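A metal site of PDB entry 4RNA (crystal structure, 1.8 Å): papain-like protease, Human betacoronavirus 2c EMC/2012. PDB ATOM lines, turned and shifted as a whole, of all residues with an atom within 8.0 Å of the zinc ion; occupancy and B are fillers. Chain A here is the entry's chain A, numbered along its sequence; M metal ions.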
ATOM      1  N   TRP A 192      21.600  19.581  -1.700  1.00  0.00           N
ATOM      2  CA  TRP A 192      20.380  20.077  -2.372  1.00  0.00           C
ATOM      3  C   TRP A 192      19.433  19.015  -2.842  1.00  0.00           C
ATOM      4  O   TRP A 192      19.803  17.847  -3.073  1.00  0.00           O
ATOM      5  CB  TRP A 192      20.712  21.074  -3.503  1.00  0.00           C
ATOM      6  CG  TRP A 192      21.187  20.384  -4.733  1.00  0.00           C
ATOM      7  CD1 TRP A 192      20.445  20.061  -5.890  1.00  0.00           C
ATOM      8  CD2 TRP A 192      22.527  19.799  -4.965  1.00  0.00           C
ATOM      9  NE1 TRP A 192      21.206  19.370  -6.793  1.00  0.00           N
ATOM     10  CE2 TRP A 192      22.470  19.164  -6.300  1.00  0.00           C
ATOM     11  CE3 TRP A 192      23.704  19.714  -4.210  1.00  0.00           C
ATOM     12  CZ2 TRP A 192      23.570  18.501  -6.849  1.00  0.00           C
ATOM     13  CZ3 TRP A 192      24.823  19.040  -4.760  1.00  0.00           C
ATOM     14  CH2 TRP A 192      24.776  18.491  -6.067  1.00  0.00           C
ATOM     15  N   CYS A 193      18.186  19.459  -2.931  1.00  0.00           N
ATOM     16  CA  CYS A 193      17.118  18.789  -3.634  1.00  0.00           C
ATOM     17  C   CYS A 193      16.443  19.837  -4.566  1.00  0.00           C
ATOM     18  O   CYS A 193      16.193  20.957  -4.139  1.00  0.00           O
ATOM     19  CB  CYS A 193      16.058  18.311  -2.639  1.00  0.00           C
ATOM     20  SG  CYS A 193      14.535  17.683  -3.421  1.00  0.00           S
ATOM     21  N   ASN A 194      16.114  19.392  -5.762  1.00  0.00           N
ATOM     22  CA  ASN A 194      15.591  20.238  -6.837  1.00  0.00           C
ATOM     23  C   ASN A 194      14.178  20.655  -6.517  1.00  0.00           C
ATOM     24  O   ASN A 194      13.697  21.672  -7.038  1.00  0.00           O
ATOM     25  CB  ASN A 194      15.792  19.531  -8.193  1.00  0.00           C
ATOM     26  CG  ASN A 194      17.274  19.337  -8.511  1.00  0.00           C
ATOM     27  OD1 ASN A 194      18.036  20.238  -8.229  1.00  0.00           O
ATOM     28  ND2 ASN A 194      17.701  18.144  -8.995  1.00  0.00           N
ATOM     29  N   VAL A 195      13.564  19.936  -5.559  1.00  0.00           N
ATOM     30  CA  VAL A 195      12.263  20.369  -4.954  1.00  0.00           C
ATOM     31  C   VAL A 195      12.417  21.139  -3.617  1.00  0.00           C
ATOM     32  O   VAL A 195      11.908  22.241  -3.448  1.00  0.00           O
ATOM     33  CB  VAL A 195      11.297  19.144  -4.808  1.00  0.00           C
ATOM     34  CG1 VAL A 195      10.050  19.503  -4.014  1.00  0.00           C
ATOM     35  CG2 VAL A 195      10.906  18.585  -6.187  1.00  0.00           C
ATOM     36  N   CYS A 196      13.183  20.580  -2.671  1.00  0.00           N
ATOM     37  CA  CYS A 196      13.249  21.105  -1.294  1.00  0.00           C
ATOM     38  C   CYS A 196      14.124  22.323  -1.105  1.00  0.00           C
ATOM     39  O   CYS A 196      13.896  23.075  -0.160  1.00  0.00           O
ATOM     40  CB  CYS A 196      13.647  19.982  -0.306  1.00  0.00           C
ATOM     41  SG  CYS A 196      12.417  18.643  -0.445  1.00  0.00           S
ATOM     42  N   GLY A 197      15.130  22.528  -1.950  1.00  0.00           N
ATOM     43  CA  GLY A 197      16.037  23.649  -1.771  1.00  0.00           C
ATOM     44  C   GLY A 197      17.484  23.260  -1.473  1.00  0.00           C
ATOM     45  O   GLY A 197      17.901  22.084  -1.586  1.00  0.00           O
ATOM     46  N   TYR A 226      21.210  10.527  -2.101  1.00  0.00           N
ATOM     47  CA  TYR A 226      20.429   9.485  -1.387  1.00  0.00           C
ATOM     48  C   TYR A 226      18.961  10.010  -1.337  1.00  0.00           C
ATOM     49  O   TYR A 226      18.666  11.052  -1.978  1.00  0.00           O
ATOM     50  CB  TYR A 226      21.052   9.187   0.001  1.00  0.00           C
ATOM     51  CG  TYR A 226      21.216  10.471   0.804  1.00  0.00           C
ATOM     52  CD1 TYR A 226      22.341  11.327   0.589  1.00  0.00           C
ATOM     53  CD2 TYR A 226      20.277  10.832   1.754  1.00  0.00           C
ATOM     54  CE1 TYR A 226      22.469  12.522   1.306  1.00  0.00           C
ATOM     55  CE2 TYR A 226      20.387  12.017   2.452  1.00  0.00           C
ATOM     56  CZ  TYR A 226      21.490  12.849   2.238  1.00  0.00           C
ATOM     57  OH  TYR A 226      21.564  14.001   2.999  1.00  0.00           O
ATOM     58  N   VAL A 227      18.060   9.302  -0.625  1.00  0.00           N
ATOM     59  CA  VAL A 227      16.623   9.580  -0.671  1.00  0.00           C
ATOM     60  C   VAL A 227      16.425  10.901   0.039  1.00  0.00           C
ATOM     61  O   VAL A 227      17.062  11.153   1.093  1.00  0.00           O
ATOM     62  CB  VAL A 227      15.758   8.433  -0.041  1.00  0.00           C
ATOM     63  CG1 VAL A 227      14.309   8.876   0.120  1.00  0.00           C
ATOM     64  CG2 VAL A 227      15.878   7.172  -0.889  1.00  0.00           C
ATOM     65  N   CYS A 228      15.637  11.757  -0.593  1.00  0.00           N
ATOM     66  CA  CYS A 228      15.229  13.016   0.039  1.00  0.00           C
ATOM     67  C   CYS A 228      13.960  12.766   0.868  1.00  0.00           C
ATOM     68  O   CYS A 228      13.193  11.851   0.556  1.00  0.00           O
ATOM     69  CB  CYS A 228      15.014  14.140  -0.948  1.00  0.00           C
ATOM     70  SG  CYS A 228      14.763  15.648   0.030  1.00  0.00           S
ATOM     71  N   GLN A 229      13.777  13.553   1.930  1.00  0.00           N
ATOM     72  CA  GLN A 229      12.554  13.524   2.722  1.00  0.00           C
ATOM     73  C   GLN A 229      11.255  13.862   1.927  1.00  0.00           C
ATOM     74  O   GLN A 229      10.164  13.518   2.359  1.00  0.00           O
ATOM     75  CB  GLN A 229      12.656  14.473   3.917  1.00  0.00           C
ATOM     76  CG  GLN A 229      12.901  15.934   3.580  1.00  0.00           C
ATOM     77  CD  GLN A 229      14.396  16.321   3.388  1.00  0.00           C
ATOM     78  OE1 GLN A 229      15.374  15.473   3.449  1.00  0.00           O
ATOM     79  NE2 GLN A 229      14.585  17.624   3.128  1.00  0.00           N
ATOM     80  N   CYS A 230      11.356  14.510   0.765  1.00  0.00           N
ATOM     81  CA  CYS A 230      10.139  14.721  -0.041  1.00  0.00           C
ATOM     82  C   CYS A 230       9.720  13.466  -0.802  1.00  0.00           C
ATOM     83  O   CYS A 230       8.672  13.450  -1.511  1.00  0.00           O
ATOM     84  CB  CYS A 230      10.394  15.870  -1.032  1.00  0.00           C
ATOM     85  SG  CYS A 230      11.705  15.433  -2.238  1.00  0.00           S
ATOM     86  N   GLY A 231      10.514  12.398  -0.726  1.00  0.00           N
ATOM     87  CA  GLY A 231      10.270  11.230  -1.579  1.00  0.00           C
ATOM     88  C   GLY A 231      11.169  11.192  -2.824  1.00  0.00           C
ATOM     89  O   GLY A 231      11.236  10.165  -3.504  1.00  0.00           O
ATOM     90  N   GLY A 232      11.855  12.306  -3.114  1.00  0.00           N
ATOM     91  CA  GLY A 232      12.754  12.360  -4.271  1.00  0.00           C
ATOM     92  C   GLY A 232      14.207  12.008  -3.904  1.00  0.00           C
ATOM     93  O   GLY A 232      14.455  11.065  -3.123  1.00  0.00           O
ATOM     94  N   GLU A 233      15.138  12.779  -4.478  1.00  0.00           N
ATOM     95  CA  GLU A 233      16.586  12.552  -4.364  1.00  0.00           C
ATOM     96  C   GLU A 233      17.211  13.787  -3.793  1.00  0.00           C
ATOM     97  O   GLU A 233      16.738  14.900  -4.045  1.00  0.00           O
ATOM     98  CB  GLU A 233      17.225  12.391  -5.734  1.00  0.00           C
ATOM     99  CG  GLU A 233      17.359  10.964  -6.188  1.00  0.00           C
ATOM    100  CD  GLU A 233      17.956  10.872  -7.597  1.00  0.00           C
ATOM    101  OE1 GLU A 233      18.230   9.730  -8.035  1.00  0.00           O
ATOM    102  OE2 GLU A 233      18.178  11.931  -8.274  1.00  0.00           O
ATOM    103  N   ARG A 234      18.286  13.576  -3.049  1.00  0.00           N
ATOM    104  CA  ARG A 234      18.980  14.609  -2.286  1.00  0.00           C
ATOM    105  C   ARG A 234      20.455  14.422  -2.665  1.00  0.00           C
ATOM    106  O   ARG A 234      20.889  13.301  -2.750  1.00  0.00           O
ATOM    107  CB  ARG A 234      18.850  14.230  -0.809  1.00  0.00           C
ATOM    108  CG  ARG A 234      18.174  15.234   0.042  1.00  0.00           C
ATOM    109  CD  ARG A 234      18.384  14.818   1.484  1.00  0.00           C
ATOM    110  NE  ARG A 234      19.352  15.765   1.975  1.00  0.00           N
ATOM    111  CZ  ARG A 234      19.132  16.704   2.915  1.00  0.00           C
ATOM    112  NH1 ARG A 234      17.959  16.796   3.572  1.00  0.00           N
ATOM    113  NH2 ARG A 234      20.130  17.520   3.258  1.00  0.00           N
HETATM  114 ZN    ZN M   1      13.348  16.900  -1.511  1.00  0.00          ZN
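The side-chain sulfur (SG) of Cys 193 sits close to the backbone carbonyl oxygen (O) of Glu 233 (3.6 Å).
The backbone NH (N) of Gly 232 sits close to the side-chain sulfur (SG) of Cys 230 (3.3 Å).
The side-chain sulfur of Cys 228 lies close to the side-chain amide oxygen of Gln 229, at 3.5 Å.
The side-chain sulfur (SG) of Cys 193 lies close to the backbone NH (N) of Val 195 (3.3 Å).
The zinc ion is bound by SG of Cys 196 (2.2 Å), SG of Cys 230 (2.3 Å), SG of Cys 193 (2.4 Å) and SG of Cys 228 (2.4 Å).
Of the 15 residues printed, 4 come within 4 Å of the zinc ion.
Along chain A the residues within 4 Å of the zinc ion span positions 193 to 230.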
